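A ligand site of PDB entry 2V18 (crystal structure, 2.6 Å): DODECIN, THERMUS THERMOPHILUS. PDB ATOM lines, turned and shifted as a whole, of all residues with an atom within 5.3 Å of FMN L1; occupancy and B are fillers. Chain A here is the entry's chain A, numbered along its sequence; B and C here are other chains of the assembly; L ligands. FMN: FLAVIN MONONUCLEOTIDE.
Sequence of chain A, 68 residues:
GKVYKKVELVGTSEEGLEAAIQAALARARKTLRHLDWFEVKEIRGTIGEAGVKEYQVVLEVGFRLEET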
ATOM      1  N   LYS A   2       5.674  12.038 -26.019  1.00  0.00           N
ATOM      2  CA  LYS A   2       6.136  10.689 -25.688  1.00  0.00           C
ATOM      3  C   LYS A   2       4.975   9.719 -25.834  1.00  0.00           C
ATOM      4  O   LYS A   2       3.832  10.087 -25.592  1.00  0.00           O
ATOM      5  CB  LYS A   2       6.641  10.605 -24.234  1.00  0.00           C
ATOM      6  CG  LYS A   2       7.522  11.738 -23.760  1.00  0.00           C
ATOM      7  CD  LYS A   2       8.047  11.418 -22.362  1.00  0.00           C
ATOM      8  CE  LYS A   2       8.614  12.661 -21.626  1.00  0.00           C
ATOM      9  NZ  LYS A   2       7.504  13.438 -20.996  1.00  0.00           N
ATOM     10  N   TYR A   4       4.099   5.634 -24.538  1.00  0.00           N
ATOM     11  CA  TYR A   4       4.507   4.450 -23.775  1.00  0.00           C
ATOM     12  C   TYR A   4       3.697   3.256 -24.230  1.00  0.00           C
ATOM     13  O   TYR A   4       2.591   3.416 -24.756  1.00  0.00           O
ATOM     14  CB  TYR A   4       4.293   4.670 -22.274  1.00  0.00           C
ATOM     15  CG  TYR A   4       5.021   5.872 -21.712  1.00  0.00           C
ATOM     16  CD1 TYR A   4       4.502   7.137 -21.864  1.00  0.00           C
ATOM     17  CD2 TYR A   4       6.231   5.732 -21.044  1.00  0.00           C
ATOM     18  CE1 TYR A   4       5.159   8.244 -21.386  1.00  0.00           C
ATOM     19  CE2 TYR A   4       6.901   6.830 -20.550  1.00  0.00           C
ATOM     20  CZ  TYR A   4       6.355   8.092 -20.726  1.00  0.00           C
ATOM     21  OH  TYR A   4       7.008   9.197 -20.264  1.00  0.00           O
ATOM     22  N   HIS A  34      13.934   1.123 -21.365  1.00  0.00           N
ATOM     23  CA  HIS A  34      13.171   2.233 -20.792  1.00  0.00           C
ATOM     24  C   HIS A  34      11.942   1.744 -20.024  1.00  0.00           C
ATOM     25  O   HIS A  34      10.882   2.365 -20.087  1.00  0.00           O
ATOM     26  CB  HIS A  34      12.781   3.249 -21.866  1.00  0.00           C
ATOM     27  CG  HIS A  34      13.894   3.574 -22.815  1.00  0.00           C
ATOM     28  ND1 HIS A  34      15.052   4.197 -22.409  1.00  0.00           N
ATOM     29  CD2 HIS A  34      14.046   3.292 -24.137  1.00  0.00           C
ATOM     30  CE1 HIS A  34      15.881   4.286 -23.436  1.00  0.00           C
ATOM     31  NE2 HIS A  34      15.283   3.755 -24.495  1.00  0.00           N
ATOM     32  N   ASP A  36       9.707   1.650 -16.994  1.00  0.00           N
ATOM     33  CA  ASP A  36       9.459   2.760 -16.084  1.00  0.00           C
ATOM     34  C   ASP A  36       8.640   2.363 -14.856  1.00  0.00           C
ATOM     35  O   ASP A  36       9.045   2.675 -13.731  1.00  0.00           O
ATOM     36  CB  ASP A  36       8.784   3.925 -16.828  1.00  0.00           C
ATOM     37  CG  ASP A  36       9.762   4.716 -17.689  1.00  0.00           C
ATOM     38  OD1 ASP A  36      10.907   4.953 -17.256  1.00  0.00           O
ATOM     39  OD2 ASP A  36       9.374   5.144 -18.782  1.00  0.00           O
ATOM     40  N   TRP A  37       7.464   1.775 -15.053  1.00  0.00           N
ATOM     41  CA  TRP A  37       6.556   1.474 -13.944  1.00  0.00           C
ATOM     42  C   TRP A  37       5.801   0.162 -14.135  1.00  0.00           C
ATOM     43  O   TRP A  37       5.791  -0.419 -15.219  1.00  0.00           O
ATOM     44  CB  TRP A  37       5.554   2.630 -13.731  1.00  0.00           C
ATOM     45  CG  TRP A  37       4.319   2.566 -14.579  1.00  0.00           C
ATOM     46  CD1 TRP A  37       3.096   2.031 -14.236  1.00  0.00           C
ATOM     47  CD2 TRP A  37       4.169   3.063 -15.920  1.00  0.00           C
ATOM     48  NE1 TRP A  37       2.214   2.137 -15.282  1.00  0.00           N
ATOM     49  CE2 TRP A  37       2.842   2.769 -16.326  1.00  0.00           C
ATOM     50  CE3 TRP A  37       5.033   3.694 -16.820  1.00  0.00           C
ATOM     51  CZ2 TRP A  37       2.374   3.106 -17.595  1.00  0.00           C
ATOM     52  CZ3 TRP A  37       4.561   4.026 -18.076  1.00  0.00           C
ATOM     53  CH2 TRP A  37       3.242   3.735 -18.449  1.00  0.00           C
ATOM     54  N   PHE A  38       5.229  -0.347 -13.048  1.00  0.00           N
ATOM     55  CA  PHE A  38       4.394  -1.546 -13.118  1.00  0.00           C
ATOM     56  C   PHE A  38       3.101  -1.410 -12.302  1.00  0.00           C
ATOM     57  O   PHE A  38       2.937  -0.488 -11.509  1.00  0.00           O
ATOM     58  CB  PHE A  38       5.202  -2.788 -12.700  1.00  0.00           C
ATOM     59  CG  PHE A  38       5.606  -2.799 -11.252  1.00  0.00           C
ATOM     60  CD1 PHE A  38       4.813  -3.429 -10.302  1.00  0.00           C
ATOM     61  CD2 PHE A  38       6.820  -2.289 -10.850  1.00  0.00           C
ATOM     62  CE1 PHE A  38       5.180  -3.469  -8.975  1.00  0.00           C
ATOM     63  CE2 PHE A  38       7.217  -2.352  -9.515  1.00  0.00           C
ATOM     64  CZ  PHE A  38       6.388  -2.944  -8.584  1.00  0.00           C
ATOM     65  N   GLU A  39       2.118  -2.240 -12.623  1.00  0.00           N
ATOM     66  CA  GLU A  39       0.817  -2.227 -11.962  1.00  0.00           C
ATOM     67  C   GLU A  39       0.411  -3.666 -11.733  1.00  0.00           C
ATOM     68  O   GLU A  39       0.303  -4.432 -12.693  1.00  0.00           O
ATOM     69  CB  GLU A  39      -0.241  -1.550 -12.831  1.00  0.00           C
ATOM     70  CG  GLU A  39       0.128  -0.156 -13.356  1.00  0.00           C
ATOM     71  CD  GLU A  39      -0.950   0.448 -14.256  1.00  0.00           C
ATOM     72  OE1 GLU A  39      -2.064  -0.143 -14.354  1.00  0.00           O
ATOM     73  OE2 GLU A  39      -0.668   1.507 -14.854  1.00  0.00           O
ATOM     74  N   ARG A  64       8.785   3.317 -22.112  1.00  0.00           N
ATOM     75  CA  ARG A  64       8.751   4.368 -23.131  1.00  0.00           C
ATOM     76  C   ARG A  64       9.180   3.813 -24.475  1.00  0.00           C
ATOM     77  O   ARG A  64      10.222   3.158 -24.583  1.00  0.00           O
ATOM     78  CB  ARG A  64       9.658   5.559 -22.769  1.00  0.00           C
ATOM     79  CG  ARG A  64       9.415   6.771 -23.689  1.00  0.00           C
ATOM     80  CD  ARG A  64      10.198   8.008 -23.303  1.00  0.00           C
ATOM     81  NE  ARG A  64      11.527   8.036 -23.926  1.00  0.00           N
ATOM     82  CZ  ARG A  64      12.672   7.634 -23.353  1.00  0.00           C
ATOM     83  NH1 ARG A  64      12.708   7.149 -22.107  1.00  0.00           N
ATOM     84  NH2 ARG A  64      13.806   7.731 -24.039  1.00  0.00           N
ATOM     85  N   ARG B  44       1.397  -0.855  -7.045  1.00  0.00           N
ATOM     86  CA  ARG B  44       2.128  -0.335  -8.204  1.00  0.00           C
ATOM     87  C   ARG B  44       3.586  -0.198  -7.814  1.00  0.00           C
ATOM     88  O   ARG B  44       3.966  -0.577  -6.706  1.00  0.00           O
ATOM     89  CB  ARG B  44       1.575   1.037  -8.611  1.00  0.00           C
ATOM     90  CG  ARG B  44       0.077   1.085  -8.829  1.00  0.00           C
ATOM     91  CD  ARG B  44      -0.419   2.506  -8.980  1.00  0.00           C
ATOM     92  NE  ARG B  44      -0.041   3.110 -10.251  1.00  0.00           N
ATOM     93  CZ  ARG B  44      -0.732   3.017 -11.383  1.00  0.00           C
ATOM     94  NH1 ARG B  44      -1.831   2.282 -11.467  1.00  0.00           N
ATOM     95  NH2 ARG B  44      -0.277   3.610 -12.469  1.00  0.00           N
ATOM     96  N   GLY B  45       4.401   0.367  -8.704  1.00  0.00           N
ATOM     97  CA  GLY B  45       5.801   0.613  -8.382  1.00  0.00           C
ATOM     98  C   GLY B  45       6.612   1.047  -9.575  1.00  0.00           C
ATOM     99  O   GLY B  45       6.103   1.083 -10.693  1.00  0.00           O
ATOM    100  N   THR B  46       7.882   1.348  -9.335  1.00  0.00           N
ATOM    101  CA  THR B  46       8.803   1.779 -10.386  1.00  0.00           C
ATOM    102  C   THR B  46       9.858   0.716 -10.630  1.00  0.00           C
ATOM    103  O   THR B  46      10.053  -0.178  -9.807  1.00  0.00           O
ATOM    104  CB  THR B  46       9.499   3.111 -10.017  1.00  0.00           C
ATOM    105  OG1 THR B  46      10.101   2.976  -8.734  1.00  0.00           O
ATOM    106  CG2 THR B  46       8.503   4.243  -9.958  1.00  0.00           C
ATOM    107  N   GLN B  56       4.922   0.568  -4.262  1.00  0.00           N
ATOM    108  CA  GLN B  56       3.942   1.626  -3.963  1.00  0.00           C
ATOM    109  C   GLN B  56       2.558   1.040  -3.717  1.00  0.00           C
ATOM    110  O   GLN B  56       1.859   0.693  -4.673  1.00  0.00           O
ATOM    111  CB  GLN B  56       3.900   2.638  -5.114  1.00  0.00           C
ATOM    112  CG  GLN B  56       5.238   3.356  -5.355  1.00  0.00           C
ATOM    113  CD  GLN B  56       5.259   4.144  -6.656  1.00  0.00           C
ATOM    114  OE1 GLN B  56       4.377   4.016  -7.471  1.00  0.00           O
ATOM    115  NE2 GLN B  56       6.310   4.918  -6.856  1.00  0.00           N
ATOM    116  N   VAL C  10       0.057   4.303 -24.135  1.00  0.00           N
ATOM    117  CA  VAL C  10      -0.231   5.521 -23.373  1.00  0.00           C
ATOM    118  C   VAL C  10       0.302   6.713 -24.161  1.00  0.00           C
ATOM    119  O   VAL C  10       1.511   6.906 -24.284  1.00  0.00           O
ATOM    120  CB  VAL C  10       0.415   5.497 -21.954  1.00  0.00           C
ATOM    121  CG1 VAL C  10       0.006   6.732 -21.155  1.00  0.00           C
ATOM    122  CG2 VAL C  10       0.062   4.226 -21.211  1.00  0.00           C
ATOM    123  N   THR C  12       0.896  10.665 -24.649  1.00  0.00           N
ATOM    124  CA  THR C  12       1.089  11.823 -23.782  1.00  0.00           C
ATOM    125  C   THR C  12       1.218  13.117 -24.595  1.00  0.00           C
ATOM    126  O   THR C  12       1.698  13.096 -25.726  1.00  0.00           O
ATOM    127  CB  THR C  12       2.345  11.671 -22.844  1.00  0.00           C
ATOM    128  OG1 THR C  12       3.550  11.873 -23.590  1.00  0.00           O
ATOM    129  CG2 THR C  12       2.396  10.316 -22.208  1.00  0.00           C
ATOM    130  N   ARG C  44      -4.958  10.118 -17.157  1.00  0.00           N
ATOM    131  CA  ARG C  44      -4.104  10.482 -16.040  1.00  0.00           C
ATOM    132  C   ARG C  44      -3.254  11.655 -16.494  1.00  0.00           C
ATOM    133  O   ARG C  44      -3.432  12.172 -17.587  1.00  0.00           O
ATOM    134  CB  ARG C  44      -3.193   9.311 -15.657  1.00  0.00           C
ATOM    135  CG  ARG C  44      -3.921   8.012 -15.380  1.00  0.00           C
ATOM    136  CD  ARG C  44      -2.955   6.865 -15.236  1.00  0.00           C
ATOM    137  NE  ARG C  44      -2.199   6.905 -13.983  1.00  0.00           N
ATOM    138  CZ  ARG C  44      -2.610   6.392 -12.819  1.00  0.00           C
ATOM    139  NH1 ARG C  44      -3.798   5.827 -12.671  1.00  0.00           N
ATOM    140  NH2 ARG C  44      -1.821   6.479 -11.750  1.00  0.00           N
ATOM    141  N   GLN C  56      -2.051  12.334 -20.095  1.00  0.00           N
ATOM    142  CA  GLN C  56      -1.670  10.949 -20.384  1.00  0.00           C
ATOM    143  C   GLN C  56      -2.910  10.059 -20.589  1.00  0.00           C
ATOM    144  O   GLN C  56      -3.594   9.667 -19.635  1.00  0.00           O
ATOM    145  CB  GLN C  56      -0.775  10.398 -19.263  1.00  0.00           C
ATOM    146  CG  GLN C  56       0.545  11.177 -19.054  1.00  0.00           C
ATOM    147  CD  GLN C  56       1.269  10.798 -17.790  1.00  0.00           C
ATOM    148  OE1 GLN C  56       0.709  10.136 -16.926  1.00  0.00           O
ATOM    149  NE2 GLN C  56       2.501  11.234 -17.665  1.00  0.00           N
ATOM    150  N   VAL C  58      -4.390   6.579 -21.450  1.00  0.00           N
ATOM    151  CA  VAL C  58      -4.129   5.156 -21.566  1.00  0.00           C
ATOM    152  C   VAL C  58      -5.197   4.577 -22.481  1.00  0.00           C
ATOM    153  O   VAL C  58      -6.392   4.656 -22.187  1.00  0.00           O
ATOM    154  CB  VAL C  58      -4.150   4.428 -20.205  1.00  0.00           C
ATOM    155  CG1 VAL C  58      -3.863   2.930 -20.380  1.00  0.00           C
ATOM    156  CG2 VAL C  58      -3.166   5.060 -19.245  1.00  0.00           C
HETATM  157  N1  FMN L   1       5.482   6.496 -11.798  1.00  0.00           N
HETATM  158  C2  FMN L   1       5.436   5.961 -10.535  1.00  0.00           C
HETATM  159  O2  FMN L   1       6.354   6.173  -9.736  1.00  0.00           O
HETATM  160  N3  FMN L   1       4.362   5.190 -10.147  1.00  0.00           N
HETATM  161  C4  FMN L   1       3.330   4.919 -11.012  1.00  0.00           C
HETATM  162  O4  FMN L   1       2.697   3.885 -10.825  1.00  0.00           O
HETATM  163  C4A FMN L   1       3.358   5.495 -12.280  1.00  0.00           C
HETATM  164  N5  FMN L   1       2.308   5.308 -13.165  1.00  0.00           N
HETATM  165  C5A FMN L   1       2.341   5.860 -14.432  1.00  0.00           C
HETATM  166  C6  FMN L   1       1.257   5.639 -15.307  1.00  0.00           C
HETATM  167  C7  FMN L   1       1.253   6.187 -16.578  1.00  0.00           C
HETATM  168  C7M FMN L   1      -0.030   6.214 -17.351  1.00  0.00           C
HETATM  169  C8  FMN L   1       2.353   6.947 -16.995  1.00  0.00           C
HETATM  170  C8M FMN L   1       2.496   7.408 -18.422  1.00  0.00           C
HETATM  171  C9  FMN L   1       3.420   7.172 -16.122  1.00  0.00           C
HETATM  172  C9A FMN L   1       3.428   6.626 -14.835  1.00  0.00           C
HETATM  173  N10 FMN L   1       4.471   6.825 -13.931  1.00  0.00           N
HETATM  174  C10 FMN L   1       4.444   6.269 -12.671  1.00  0.00           C
HETATM  175  C1' FMN L   1       5.548   7.818 -14.208  1.00  0.00           C
HETATM  176  C2' FMN L   1       6.587   7.163 -15.104  1.00  0.00           C
HETATM  177  O2' FMN L   1       7.432   6.408 -14.270  1.00  0.00           O
HETATM  178  C3' FMN L   1       7.274   8.275 -15.890  1.00  0.00           C
HETATM  179  O3' FMN L   1       7.008   8.175 -17.282  1.00  0.00           O
HETATM  180  C4' FMN L   1       8.767   8.281 -15.670  1.00  0.00           C
HETATM  181  O4' FMN L   1       8.950   8.479 -14.279  1.00  0.00           O
HETATM  182  C5' FMN L   1       9.388   9.380 -16.524  1.00  0.00           C
HETATM  183  O5' FMN L   1       9.124   9.133 -17.899  1.00  0.00           O
HETATM  184  P   FMN L   1      10.291   8.925 -18.995  1.00  0.00           P
HETATM  185  O1P FMN L   1       9.931   9.808 -20.172  1.00  0.00           O
HETATM  186  O2P FMN L   1      11.595   9.395 -18.385  1.00  0.00           O
HETATM  187  O3P FMN L   1      10.410   7.480 -19.441  1.00  0.00           O
HETATM  188  N1  FMN L   2       3.463   9.792 -12.657  1.00  0.00           N
HETATM  189  C2  FMN L   2       2.927  10.016 -13.914  1.00  0.00           C
HETATM  190  O2  FMN L   2       3.540  10.676 -14.743  1.00  0.00           O
HETATM  191  N3  FMN L   2       1.690   9.485 -14.244  1.00  0.00           N
HETATM  192  C4  FMN L   2       0.959   8.744 -13.335  1.00  0.00           C
HETATM  193  O4  FMN L   2      -0.265   8.828 -13.432  1.00  0.00           O
HETATM  194  C4A FMN L   2       1.509   8.478 -12.089  1.00  0.00           C
HETATM  195  N5  FMN L   2       0.802   7.747 -11.163  1.00  0.00           N
HETATM  196  C5A FMN L   2       1.321   7.507  -9.900  1.00  0.00           C
HETATM  197  C6  FMN L   2       0.614   6.721  -8.993  1.00  0.00           C
HETATM  198  C7  FMN L   2       1.125   6.454  -7.727  1.00  0.00           C
HETATM  199  C7M FMN L   2       0.507   5.372  -6.904  1.00  0.00           C
HETATM  200  C8  FMN L   2       2.367   7.003  -7.358  1.00  0.00           C
HETATM  201  C8M FMN L   2       2.861   6.925  -5.942  1.00  0.00           C
HETATM  202  C9  FMN L   2       3.082   7.770  -8.277  1.00  0.00           C
HETATM  203  C9A FMN L   2       2.578   8.034  -9.551  1.00  0.00           C
HETATM  204  N10 FMN L   2       3.276   8.796 -10.484  1.00  0.00           N
HETATM  205  C10 FMN L   2       2.744   9.033 -11.743  1.00  0.00           C
HETATM  206  C1' FMN L   2       4.683   9.219 -10.266  1.00  0.00           C
HETATM  207  C2' FMN L   2       4.679  10.455  -9.397  1.00  0.00           C
HETATM  208  O2' FMN L   2       4.399  11.589 -10.208  1.00  0.00           O
HETATM  209  C3' FMN L   2       6.029  10.477  -8.666  1.00  0.00           C
HETATM  210  O3' FMN L   2       5.846  10.311  -7.265  1.00  0.00           O
HETATM  211  C4' FMN L   2       6.803  11.740  -8.944  1.00  0.00           C
HETATM  212  O4' FMN L   2       7.085  11.783 -10.332  1.00  0.00           O
HETATM  213  C5' FMN L   2       8.090  11.711  -8.123  1.00  0.00           C
HETATM  214  O5' FMN L   2       7.730  11.657  -6.758  1.00  0.00           O
HETATM  215  P   FMN L   2       8.198  12.766  -5.693  1.00  0.00           P
HETATM  216  O1P FMN L   2       8.810  12.003  -4.534  1.00  0.00           O
HETATM  217  O2P FMN L   2       9.279  13.607  -6.355  1.00  0.00           O
HETATM  218  O3P FMN L   2       7.038  13.612  -5.206  1.00  0.00           O
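The backbone carbonyl oxygen (O) of His 34 lies within hydrogen-bond range of the backbone NH (N) of Arg 64, at 3.1 Å. The backbone carbonyl oxygen (O) of Tyr 4 is in hydrogen-bond range of the backbone NH (N) of Val 10 of chain C (2.8 Å). The backbone carbonyl oxygen of Gln 56 of chain C is in hydrogen-bond range of the backbone NH of Arg 44 of chain C, at 2.9 Å. NH2 of Arg 44 of chain B is in salt-bridge range of OE2 of Glu 39, at 3.2 Å. The indole nitrogen (NE1) of Trp 37 sits at hydrogen-bond distance from the side-chain carboxylate (OE2) of Glu 39, 3.0 Å away. The side-chain hydroxyl of Thr 12 of chain C is in hydrogen-bond range of the backbone carbonyl oxygen of Lys 2, 2.7 Å away. O of Arg 44 of chain B lies within hydrogen-bond range of N of Gln 56 of chain B (2.9 Å).
NE of Arg 44 of chain C is in hydrogen-bond range of O4 of FMN L2 (2.8 Å). An oxygen (O4) of FMN L1 sits at hydrogen-bond distance from the guanidinium group of Arg 44 of chain B, 2.9 Å away. N3 of FMN L2 sits at hydrogen-bond distance from OE1 of Gln 56 of chain C (2.9 Å). The side-chain amide oxygen (OE1) of Gln 56 of chain B lies within hydrogen-bond range of a nitrogen (N3) of FMN L1. OD2 of Asp 36 lies close to O3P of FMN L1 (2.6 Å). The side-chain hydroxyl (OH) of Tyr 4 lies within hydrogen-bond range of an oxygen (O1P) of FMN L1, at 3.0 Å. An oxygen (O3P) of FMN L1 is in salt-bridge range of the guanidinium group (NH1) of Arg 64, 3.5 Å away.
Merely in contact with FMN L1: Thr 46 of chain B (2.9 Å), Lys 2 (3.3 Å), Trp 37 (3.4 Å), Gln 56 of chain C (3.6 Å), Arg 44 of chain C (3.7 Å), Val 10 of chain C (3.8 Å) and Val 58 of chain C (3.8 Å). Hydrophobic or aromatic side chains within 4 Å of FMN L1: Tyr 4, Trp 37, Val 10 of chain C and Val 58 of chain C. Of the 17 residues printed, 12 come within 4 Å of FMN L1. The nearest printed residue that does not touch FMN L1 is Gly 45 of chain B (4.4 Å).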
